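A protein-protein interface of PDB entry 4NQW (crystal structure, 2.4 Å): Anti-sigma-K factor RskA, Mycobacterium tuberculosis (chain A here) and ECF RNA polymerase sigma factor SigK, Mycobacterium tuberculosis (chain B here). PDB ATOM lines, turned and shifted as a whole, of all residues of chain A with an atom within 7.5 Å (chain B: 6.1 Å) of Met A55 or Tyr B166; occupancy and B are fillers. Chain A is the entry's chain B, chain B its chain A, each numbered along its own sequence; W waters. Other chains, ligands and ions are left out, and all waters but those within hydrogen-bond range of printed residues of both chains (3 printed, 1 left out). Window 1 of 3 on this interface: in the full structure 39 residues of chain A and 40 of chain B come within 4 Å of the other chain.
The backbone carbonyl oxygen (O) of Leu A18 is in hydrogen-bond range of a ring nitrogen (NE2) of His B102, 3.3 Å away.
N of Leu B170 lies within hydrogen-bond range of O of Leu B164. A ring nitrogen (NE2) of His B102 sits close to the backbone carbonyl oxygen (O) of Tyr B166 (3.3 Å). The backbone carbonyl oxygen of Ser A59 sits at hydrogen-bond distance from the side-chain hydroxyl of Thr A62. O of Ala A50 lies within hydrogen-bond range of OG1 of Thr A54 (2.8 Å). N of Leu B170 is in hydrogen-bond range of O of Ala B165. O of Ile B162 sits at hydrogen-bond distance from N of Tyr B167 (3.4 Å).
Among the printed residues, pairs that only touch across the chains: Leu A18 with Tyr B166, Asn A19 with His B102, Ala A20 with Leu B170, Val A51 with Leu B194, Thr A54 with Leu B197, Met A55 with Tyr B166, Met A55 with Leu B194, Val A58 with Tyr B167 and Thr A62 with Tyr B167.
Of the printed residues of chain B, Asn A19 touches His B102. Printed residues of chain B within 4 Å of Ala A20: Leu B170 (3.8 Å). Ala A50 touches none of the printed residues of chain B. Printed residues of chain B within 4 Å of Thr A54: Leu B197. Of chain B, only Tyr B166 (3.4 Å) and Leu B194 (3.8 Å) come within 4 Å of Met A55. Of the printed residues of chain B, Val A58 touches Tyr B167 (3.9 Å). Ala B165 touches none of the printed residues of chain A. Tyr B166 touches two residues of chain A. Of the printed residues of chain A, Leu B170 touches Ala A20 (3.8 Å). The nearest residue of chain B that does not touch Met A55 is Ile B162 (4.4 Å).
Hydrophobic or aromatic side chains of chain B that line the printed part of chain A: His B102, Tyr B166, Tyr B167, Leu B194 and Leu B197. Along chain B the printed residues that touch a printed residue of chain A span positions 102 to 197. Printed residues of chain A that touch a printed residue of chain B: Leu A18, Asn A19, Ala A20, Val A51, Thr A54, Met A55, Val A58 and Thr A62. Hydrophobic or aromatic side chains of chain A that line the printed part of chain B: Leu A18, Ala A20, Val A51, Met A55 and Val A58. Among the printed residues, 10 pairs touch across the chains.
Water W2 bridges the side-chain hydroxyl (OH) of Tyr B167 (2.5 Å) and the side-chain hydroxyl (OG1) of Thr A62 (2.8 Å). Water W3 lies within hydrogen-bond range of the side-chain hydroxyl of Thr A62 (2.6 Å), the backbone carbonyl oxygen of Ser A59 (2.7 Å) and the backbone NH of Leu B57 (3.3 Å). Water W1 lies within hydrogen-bond range of OH of Tyr B166 (2.7 Å), O of Met A55 (2.8 Å) and N of Ser A59 (3.3 Å).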
ATOM      1  N   ALA A  17       9.195   8.035   0.027  1.00  0.00           N
ATOM      2  CA  ALA A  17       8.732   7.280  -1.145  1.00  0.00           C
ATOM      3  C   ALA A  17       7.215   7.083  -1.171  1.00  0.00           C
ATOM      4  O   ALA A  17       6.619   6.979  -2.244  1.00  0.00           O
ATOM      5  CB  ALA A  17       9.435   5.932  -1.218  1.00  0.00           C
ATOM      6  N   LEU A  18       6.597   7.038   0.008  1.00  0.00           N
ATOM      7  CA  LEU A  18       5.145   6.933   0.120  1.00  0.00           C
ATOM      8  C   LEU A  18       4.446   8.294   0.052  1.00  0.00           C
ATOM      9  O   LEU A  18       3.225   8.369   0.201  1.00  0.00           O
ATOM     10  CB  LEU A  18       4.775   6.247   1.434  1.00  0.00           C
ATOM     11  CG  LEU A  18       5.348   4.844   1.630  1.00  0.00           C
ATOM     12  CD1 LEU A  18       5.176   4.405   3.077  1.00  0.00           C
ATOM     13  CD2 LEU A  18       4.691   3.860   0.674  1.00  0.00           C
ATOM     14  N   ASN A  19       5.215   9.359  -0.180  1.00  0.00           N
ATOM     15  CA  ASN A  19       4.709  10.734  -0.112  1.00  0.00           C
ATOM     16  C   ASN A  19       4.112  11.029   1.265  1.00  0.00           C
ATOM     17  O   ASN A  19       3.183  11.831   1.396  1.00  0.00           O
ATOM     18  CB  ASN A  19       3.703  11.011  -1.240  1.00  0.00           C
ATOM     19  CG  ASN A  19       4.338  10.927  -2.619  1.00  0.00           C
ATOM     20  OD1 ASN A  19       5.174  11.754  -2.973  1.00  0.00           O
ATOM     21  ND2 ASN A  19       3.946   9.929  -3.402  1.00  0.00           N
ATOM     22  N   ALA A  20       4.682  10.385   2.285  1.00  0.00           N
ATOM     23  CA  ALA A  20       4.226  10.496   3.667  1.00  0.00           C
ATOM     24  C   ALA A  20       5.067  11.505   4.452  1.00  0.00           C
ATOM     25  O   ALA A  20       5.287  11.341   5.652  1.00  0.00           O
ATOM     26  CB  ALA A  20       4.266   9.132   4.341  1.00  0.00           C
ATOM     27  N   ARG A  49      13.537   3.966  -4.344  1.00  0.00           N
ATOM     28  CA  ARG A  49      13.176   3.236  -5.555  1.00  0.00           C
ATOM     29  C   ARG A  49      12.462   1.933  -5.215  1.00  0.00           C
ATOM     30  O   ARG A  49      11.373   1.674  -5.717  1.00  0.00           O
ATOM     31  CB  ARG A  49      14.423   2.950  -6.395  1.00  0.00           C
ATOM     32  CG  ARG A  49      14.162   2.201  -7.697  1.00  0.00           C
ATOM     33  CD  ARG A  49      15.412   1.491  -8.197  1.00  0.00           C
ATOM     34  NE  ARG A  49      16.002   0.638  -7.162  1.00  0.00           N
ATOM     35  CZ  ARG A  49      15.538  -0.556  -6.790  1.00  0.00           C
ATOM     36  NH1 ARG A  49      14.463  -1.088  -7.365  1.00  0.00           N
ATOM     37  NH2 ARG A  49      16.164  -1.232  -5.831  1.00  0.00           N
ATOM     38  N   ALA A  50      13.074   1.128  -4.349  1.00  0.00           N
ATOM     39  CA  ALA A  50      12.519  -0.176  -3.972  1.00  0.00           C
ATOM     40  C   ALA A  50      11.086  -0.071  -3.442  1.00  0.00           C
ATOM     41  O   ALA A  50      10.253  -0.931  -3.724  1.00  0.00           O
ATOM     42  CB  ALA A  50      13.414  -0.853  -2.942  1.00  0.00           C
ATOM     43  N   VAL A  51      10.813   0.986  -2.678  1.00  0.00           N
ATOM     44  CA  VAL A  51       9.476   1.239  -2.139  1.00  0.00           C
ATOM     45  C   VAL A  51       8.489   1.611  -3.248  1.00  0.00           C
ATOM     46  O   VAL A  51       7.356   1.127  -3.253  1.00  0.00           O
ATOM     47  CB  VAL A  51       9.505   2.342  -1.051  1.00  0.00           C
ATOM     48  CG1 VAL A  51       8.107   2.866  -0.743  1.00  0.00           C
ATOM     49  CG2 VAL A  51      10.152   1.807   0.217  1.00  0.00           C
ATOM     50  N   ARG A  52       8.922   2.452  -4.187  1.00  0.00           N
ATOM     51  CA  ARG A  52       8.052   2.885  -5.285  1.00  0.00           C
ATOM     52  C   ARG A  52       7.669   1.681  -6.144  1.00  0.00           C
ATOM     53  O   ARG A  52       6.518   1.556  -6.561  1.00  0.00           O
ATOM     54  CB  ARG A  52       8.707   3.942  -6.193  1.00  0.00           C
ATOM     55  CG  ARG A  52       9.566   5.012  -5.527  1.00  0.00           C
ATOM     56  CD  ARG A  52       8.856   6.317  -5.202  1.00  0.00           C
ATOM     57  NE  ARG A  52       9.703   7.466  -5.540  1.00  0.00           N
ATOM     58  CZ  ARG A  52       9.532   8.713  -5.095  1.00  0.00           C
ATOM     59  NH1 ARG A  52       8.537   9.021  -4.267  1.00  0.00           N
ATOM     60  NH2 ARG A  52      10.371   9.667  -5.488  1.00  0.00           N
ATOM     61  N   GLU A  53       8.640   0.805  -6.412  1.00  0.00           N
ATOM     62  CA  GLU A  53       8.395  -0.396  -7.219  1.00  0.00           C
ATOM     63  C   GLU A  53       7.371  -1.288  -6.523  1.00  0.00           C
ATOM     64  O   GLU A  53       6.404  -1.733  -7.141  1.00  0.00           O
ATOM     65  CB  GLU A  53       9.684  -1.198  -7.461  1.00  0.00           C
ATOM     66  CG  GLU A  53      10.831  -0.444  -8.132  1.00  0.00           C
ATOM     67  CD  GLU A  53      10.501   0.094  -9.515  1.00  0.00           C
ATOM     68  OE1 GLU A  53       9.648  -0.493 -10.212  1.00  0.00           O
ATOM     69  OE2 GLU A  53      11.115   1.109  -9.913  1.00  0.00           O
ATOM     70  N   THR A  54       7.592  -1.535  -5.232  1.00  0.00           N
ATOM     71  CA  THR A  54       6.674  -2.335  -4.419  1.00  0.00           C
ATOM     72  C   THR A  54       5.246  -1.791  -4.503  1.00  0.00           C
ATOM     73  O   THR A  54       4.304  -2.545  -4.718  1.00  0.00           O
ATOM     74  CB  THR A  54       7.127  -2.381  -2.942  1.00  0.00           C
ATOM     75  OG1 THR A  54       8.441  -2.943  -2.857  1.00  0.00           O
ATOM     76  CG2 THR A  54       6.182  -3.221  -2.102  1.00  0.00           C
ATOM     77  N   MET A  55       5.092  -0.480  -4.350  1.00  0.00           N
ATOM     78  CA  MET A  55       3.764   0.129  -4.388  1.00  0.00           C
ATOM     79  C   MET A  55       3.162   0.116  -5.796  1.00  0.00           C
ATOM     80  O   MET A  55       1.944   0.007  -5.947  1.00  0.00           O
ATOM     81  CB  MET A  55       3.805   1.548  -3.821  1.00  0.00           C
ATOM     82  CG  MET A  55       4.225   1.607  -2.360  1.00  0.00           C
ATOM     83  SD  MET A  55       3.375   0.418  -1.299  1.00  0.00           S
ATOM     84  CE  MET A  55       1.711   1.079  -1.314  1.00  0.00           C
ATOM     85  N   ALA A  56       4.012   0.212  -6.816  1.00  0.00           N
ATOM     86  CA  ALA A  56       3.571   0.075  -8.207  1.00  0.00           C
ATOM     87  C   ALA A  56       3.008  -1.322  -8.470  1.00  0.00           C
ATOM     88  O   ALA A  56       2.036  -1.472  -9.215  1.00  0.00           O
ATOM     89  CB  ALA A  56       4.713   0.371  -9.166  1.00  0.00           C
ATOM     90  N   VAL A  57       3.624  -2.335  -7.862  1.00  0.00           N
ATOM     91  CA  VAL A  57       3.098  -3.700  -7.904  1.00  0.00           C
ATOM     92  C   VAL A  57       1.792  -3.772  -7.116  1.00  0.00           C
ATOM     93  O   VAL A  57       0.812  -4.357  -7.581  1.00  0.00           O
ATOM     94  CB  VAL A  57       4.107  -4.723  -7.329  1.00  0.00           C
ATOM     95  CG1 VAL A  57       3.464  -6.095  -7.159  1.00  0.00           C
ATOM     96  CG2 VAL A  57       5.338  -4.824  -8.223  1.00  0.00           C
ATOM     97  N   VAL A  58       1.788  -3.168  -5.929  1.00  0.00           N
ATOM     98  CA  VAL A  58       0.624  -3.186  -5.032  1.00  0.00           C
ATOM     99  C   VAL A  58      -0.631  -2.550  -5.656  1.00  0.00           C
ATOM    100  O   VAL A  58      -1.753  -2.926  -5.309  1.00  0.00           O
ATOM    101  CB  VAL A  58       0.957  -2.520  -3.668  1.00  0.00           C
ATOM    102  CG1 VAL A  58      -0.296  -2.221  -2.854  1.00  0.00           C
ATOM    103  CG2 VAL A  58       1.888  -3.411  -2.859  1.00  0.00           C
ATOM    104  N   SER A  59      -0.441  -1.611  -6.584  1.00  0.00           N
ATOM    105  CA  SER A  59      -1.561  -0.932  -7.254  1.00  0.00           C
ATOM    106  C   SER A  59      -2.566  -1.883  -7.917  1.00  0.00           C
ATOM    107  O   SER A  59      -3.724  -1.514  -8.118  1.00  0.00           O
ATOM    108  CB  SER A  59      -1.043   0.071  -8.292  1.00  0.00           C
ATOM    109  OG  SER A  59      -0.451  -0.586  -9.401  1.00  0.00           O
ATOM    110  N   ALA A  60      -2.129  -3.096  -8.252  1.00  0.00           N
ATOM    111  CA  ALA A  60      -3.027  -4.126  -8.792  1.00  0.00           C
ATOM    112  C   ALA A  60      -4.235  -4.403  -7.893  1.00  0.00           C
ATOM    113  O   ALA A  60      -5.284  -4.819  -8.383  1.00  0.00           O
ATOM    114  CB  ALA A  60      -2.262  -5.418  -9.034  1.00  0.00           C
ATOM    115  N   ALA A  61      -4.083  -4.176  -6.590  1.00  0.00           N
ATOM    116  CA  ALA A  61      -5.146  -4.449  -5.622  1.00  0.00           C
ATOM    117  C   ALA A  61      -6.260  -3.398  -5.624  1.00  0.00           C
ATOM    118  O   ALA A  61      -7.415  -3.729  -5.353  1.00  0.00           O
ATOM    119  CB  ALA A  61      -4.560  -4.589  -4.222  1.00  0.00           C
ATOM    120  N   THR A  62      -5.913  -2.144  -5.919  1.00  0.00           N
ATOM    121  CA  THR A  62      -6.879  -1.035  -5.901  1.00  0.00           C
ATOM    122  C   THR A  62      -7.418  -0.681  -7.289  1.00  0.00           C
ATOM    123  O   THR A  62      -8.057   0.358  -7.462  1.00  0.00           O
ATOM    124  CB  THR A  62      -6.249   0.235  -5.293  1.00  0.00           C
ATOM    125  OG1 THR A  62      -4.994   0.503  -5.933  1.00  0.00           O
ATOM    126  CG2 THR A  62      -6.034   0.061  -3.803  1.00  0.00           C
ATOM    127  N   LEU B  57      -6.247   3.894  -8.059  1.00  0.00           N
ATOM    128  CA  LEU B  57      -5.498   4.456  -6.940  1.00  0.00           C
ATOM    129  C   LEU B  57      -6.077   5.808  -6.545  1.00  0.00           C
ATOM    130  O   LEU B  57      -6.332   6.060  -5.369  1.00  0.00           O
ATOM    131  CB  LEU B  57      -4.009   4.605  -7.279  1.00  0.00           C
ATOM    132  CG  LEU B  57      -3.160   5.293  -6.201  1.00  0.00           C
ATOM    133  CD1 LEU B  57      -3.282   4.586  -4.857  1.00  0.00           C
ATOM    134  CD2 LEU B  57      -1.706   5.361  -6.631  1.00  0.00           C
ATOM    135  N   VAL B  61      -7.927   7.043  -2.991  1.00  0.00           N
ATOM    136  CA  VAL B  61      -7.459   8.144  -2.145  1.00  0.00           C
ATOM    137  C   VAL B  61      -8.515   9.244  -2.007  1.00  0.00           C
ATOM    138  O   VAL B  61      -8.813   9.681  -0.897  1.00  0.00           O
ATOM    139  CB  VAL B  61      -6.142   8.752  -2.683  1.00  0.00           C
ATOM    140  CG1 VAL B  61      -5.716   9.957  -1.853  1.00  0.00           C
ATOM    141  CG2 VAL B  61      -5.036   7.708  -2.686  1.00  0.00           C
ATOM    142  N   LEU B  98       2.884   5.712 -11.196  1.00  0.00           N
ATOM    143  CA  LEU B  98       2.067   5.551  -9.988  1.00  0.00           C
ATOM    144  C   LEU B  98       2.520   6.462  -8.848  1.00  0.00           C
ATOM    145  O   LEU B  98       1.700   6.921  -8.057  1.00  0.00           O
ATOM    146  CB  LEU B  98       2.029   4.091  -9.516  1.00  0.00           C
ATOM    147  CG  LEU B  98       0.861   3.238 -10.026  1.00  0.00           C
ATOM    148  CD1 LEU B  98      -0.484   3.827  -9.634  1.00  0.00           C
ATOM    149  CD2 LEU B  98       0.930   3.063 -11.527  1.00  0.00           C
ATOM    150  N   HIS B 102       0.085   9.114  -7.131  1.00  0.00           N
ATOM    151  CA  HIS B 102      -0.132   9.106  -5.693  1.00  0.00           C
ATOM    152  C   HIS B 102       0.177  10.461  -5.072  1.00  0.00           C
ATOM    153  O   HIS B 102      -0.566  10.950  -4.220  1.00  0.00           O
ATOM    154  CB  HIS B 102       0.746   8.052  -5.031  1.00  0.00           C
ATOM    155  CG  HIS B 102       0.472   7.888  -3.575  1.00  0.00           C
ATOM    156  ND1 HIS B 102      -0.580   7.137  -3.104  1.00  0.00           N
ATOM    157  CD2 HIS B 102       1.088   8.400  -2.484  1.00  0.00           C
ATOM    158  CE1 HIS B 102      -0.592   7.185  -1.786  1.00  0.00           C
ATOM    159  NE2 HIS B 102       0.410   7.943  -1.383  1.00  0.00           N
ATOM    160  N   VAL B 106      -2.727  12.479  -3.091  1.00  0.00           N
ATOM    161  CA  VAL B 106      -2.481  12.790  -1.681  1.00  0.00           C
ATOM    162  C   VAL B 106      -2.457  14.302  -1.462  1.00  0.00           C
ATOM    163  O   VAL B 106      -3.045  14.807  -0.505  1.00  0.00           O
ATOM    164  CB  VAL B 106      -1.162  12.144  -1.186  1.00  0.00           C
ATOM    165  CG1 VAL B 106      -0.626  12.838   0.061  1.00  0.00           C
ATOM    166  CG2 VAL B 106      -1.376  10.658  -0.925  1.00  0.00           C
ATOM    167  N   CYS B 161      -0.126   1.226   9.207  1.00  0.00           N
ATOM    168  CA  CYS B 161       0.813   2.258   8.751  1.00  0.00           C
ATOM    169  C   CYS B 161       0.609   2.598   7.280  1.00  0.00           C
ATOM    170  O   CYS B 161       0.534   3.773   6.913  1.00  0.00           O
ATOM    171  CB  CYS B 161       2.268   1.824   8.974  1.00  0.00           C
ATOM    172  SG  CYS B 161       2.882   2.137  10.643  1.00  0.00           S
ATOM    173  N   ILE B 162       0.524   1.567   6.443  1.00  0.00           N
ATOM    174  CA  ILE B 162       0.295   1.758   5.012  1.00  0.00           C
ATOM    175  C   ILE B 162      -1.105   2.322   4.761  1.00  0.00           C
ATOM    176  O   ILE B 162      -1.282   3.183   3.905  1.00  0.00           O
ATOM    177  CB  ILE B 162       0.515   0.449   4.219  1.00  0.00           C
ATOM    178  CG1 ILE B 162       1.982   0.017   4.336  1.00  0.00           C
ATOM    179  CG2 ILE B 162       0.122   0.628   2.753  1.00  0.00           C
ATOM    180  CD1 ILE B 162       2.358  -1.214   3.537  1.00  0.00           C
ATOM    181  N   GLU B 163      -2.089   1.846   5.519  1.00  0.00           N
ATOM    182  CA  GLU B 163      -3.473   2.310   5.378  1.00  0.00           C
ATOM    183  C   GLU B 163      -3.597   3.816   5.627  1.00  0.00           C
ATOM    184  O   GLU B 163      -4.227   4.530   4.843  1.00  0.00           O
ATOM    185  CB  GLU B 163      -4.395   1.549   6.338  1.00  0.00           C
ATOM    186  CG  GLU B 163      -5.876   1.622   5.988  1.00  0.00           C
ATOM    187  CD  GLU B 163      -6.265   0.687   4.854  1.00  0.00           C
ATOM    188  OE1 GLU B 163      -5.983  -0.528   4.953  1.00  0.00           O
ATOM    189  OE2 GLU B 163      -6.868   1.165   3.869  1.00  0.00           O
ATOM    190  N   LEU B 164      -2.992   4.294   6.713  1.00  0.00           N
ATOM    191  CA  LEU B 164      -3.085   5.708   7.087  1.00  0.00           C
ATOM    192  C   LEU B 164      -2.184   6.600   6.235  1.00  0.00           C
ATOM    193  O   LEU B 164      -2.618   7.649   5.762  1.00  0.00           O
ATOM    194  CB  LEU B 164      -2.752   5.898   8.571  1.00  0.00           C
ATOM    195  CG  LEU B 164      -3.750   5.301   9.569  1.00  0.00           C
ATOM    196  CD1 LEU B 164      -3.191   5.390  10.978  1.00  0.00           C
ATOM    197  CD2 LEU B 164      -5.103   5.994   9.495  1.00  0.00           C
ATOM    198  N   ALA B 165      -0.935   6.184   6.036  1.00  0.00           N
ATOM    199  CA  ALA B 165       0.034   7.000   5.304  1.00  0.00           C
ATOM    200  C   ALA B 165      -0.239   7.010   3.809  1.00  0.00           C
ATOM    201  O   ALA B 165      -0.410   8.071   3.213  1.00  0.00           O
ATOM    202  CB  ALA B 165       1.448   6.514   5.569  1.00  0.00           C
ATOM    203  N   TYR B 166      -0.279   5.823   3.211  1.00  0.00           N
ATOM    204  CA  TYR B 166      -0.422   5.698   1.766  1.00  0.00           C
ATOM    205  C   TYR B 166      -1.848   6.036   1.316  1.00  0.00           C
ATOM    206  O   TYR B 166      -2.050   7.006   0.597  1.00  0.00           O
ATOM    207  CB  TYR B 166      -0.001   4.299   1.304  1.00  0.00           C
ATOM    208  CG  TYR B 166       0.181   4.170  -0.189  1.00  0.00           C
ATOM    209  CD1 TYR B 166       1.291   4.719  -0.830  1.00  0.00           C
ATOM    210  CD2 TYR B 166      -0.751   3.486  -0.963  1.00  0.00           C
ATOM    211  CE1 TYR B 166       1.459   4.597  -2.201  1.00  0.00           C
ATOM    212  CE2 TYR B 166      -0.594   3.361  -2.332  1.00  0.00           C
ATOM    213  CZ  TYR B 166       0.510   3.917  -2.947  1.00  0.00           C
ATOM    214  OH  TYR B 166       0.661   3.788  -4.307  1.00  0.00           O
ATOM    215  N   TYR B 167      -2.838   5.265   1.758  1.00  0.00           N
ATOM    216  CA  TYR B 167      -4.220   5.495   1.318  1.00  0.00           C
ATOM    217  C   TYR B 167      -4.891   6.697   1.983  1.00  0.00           C
ATOM    218  O   TYR B 167      -5.591   7.457   1.316  1.00  0.00           O
ATOM    219  CB  TYR B 167      -5.069   4.236   1.505  1.00  0.00           C
ATOM    220  CG  TYR B 167      -4.612   3.090   0.635  1.00  0.00           C
ATOM    221  CD1 TYR B 167      -4.471   3.253  -0.741  1.00  0.00           C
ATOM    222  CD2 TYR B 167      -4.318   1.840   1.184  1.00  0.00           C
ATOM    223  CE1 TYR B 167      -4.051   2.211  -1.546  1.00  0.00           C
ATOM    224  CE2 TYR B 167      -3.895   0.788   0.384  1.00  0.00           C
ATOM    225  CZ  TYR B 167      -3.764   0.980  -0.980  1.00  0.00           C
ATOM    226  OH  TYR B 167      -3.348  -0.057  -1.780  1.00  0.00           O
ATOM    227  N   GLY B 168      -4.672   6.870   3.283  1.00  0.00           N
ATOM    228  CA  GLY B 168      -5.253   7.989   4.029  1.00  0.00           C
ATOM    229  C   GLY B 168      -4.562   9.323   3.795  1.00  0.00           C
ATOM    230  O   GLY B 168      -5.109  10.374   4.137  1.00  0.00           O
ATOM    231  N   GLY B 169      -3.357   9.286   3.230  1.00  0.00           N
ATOM    232  CA  GLY B 169      -2.611  10.498   2.894  1.00  0.00           C
ATOM    233  C   GLY B 169      -1.930  11.191   4.065  1.00  0.00           C
ATOM    234  O   GLY B 169      -1.448  12.316   3.922  1.00  0.00           O
ATOM    235  N   LEU B 170      -1.874  10.528   5.218  1.00  0.00           N
ATOM    236  CA  LEU B 170      -1.243  11.104   6.406  1.00  0.00           C
ATOM    237  C   LEU B 170       0.279  11.072   6.290  1.00  0.00           C
ATOM    238  O   LEU B 170       0.848  10.143   5.713  1.00  0.00           O
ATOM    239  CB  LEU B 170      -1.670  10.359   7.679  1.00  0.00           C
ATOM    240  CG  LEU B 170      -3.041  10.696   8.272  1.00  0.00           C
ATOM    241  CD1 LEU B 170      -4.174  10.217   7.381  1.00  0.00           C
ATOM    242  CD2 LEU B 170      -3.172  10.088   9.660  1.00  0.00           C
ATOM    243  N   LEU B 194       6.879  -2.300   4.484  1.00  0.00           N
ATOM    244  CA  LEU B 194       7.338  -2.332   3.090  1.00  0.00           C
ATOM    245  C   LEU B 194       8.336  -3.460   2.809  1.00  0.00           C
ATOM    246  O   LEU B 194       8.387  -3.967   1.689  1.00  0.00           O
ATOM    247  CB  LEU B 194       7.937  -0.981   2.675  1.00  0.00           C
ATOM    248  CG  LEU B 194       6.964   0.045   2.083  1.00  0.00           C
ATOM    249  CD1 LEU B 194       6.550  -0.348   0.673  1.00  0.00           C
ATOM    250  CD2 LEU B 194       5.740   0.256   2.961  1.00  0.00           C
ATOM    251  N   LEU B 197       6.252  -6.634   2.516  1.00  0.00           N
ATOM    252  CA  LEU B 197       5.575  -6.601   1.219  1.00  0.00           C
ATOM    253  C   LEU B 197       6.533  -6.941   0.084  1.00  0.00           C
ATOM    254  O   LEU B 197       6.212  -7.764  -0.774  1.00  0.00           O
ATOM    255  CB  LEU B 197       4.934  -5.231   0.961  1.00  0.00           C
ATOM    256  CG  LEU B 197       3.623  -4.918   1.683  1.00  0.00           C
ATOM    257  CD1 LEU B 197       3.110  -3.560   1.234  1.00  0.00           C
ATOM    258  CD2 LEU B 197       2.577  -5.993   1.431  1.00  0.00           C
HETATM  259  O   HOH W   1      -0.322   1.442  -5.264  1.00  0.00           O
HETATM  260  O   HOH W   2      -2.810   0.471  -4.174  1.00  0.00           O
HETATM  261  O   HOH W   3      -4.929   0.919  -8.540  1.00  0.00           O
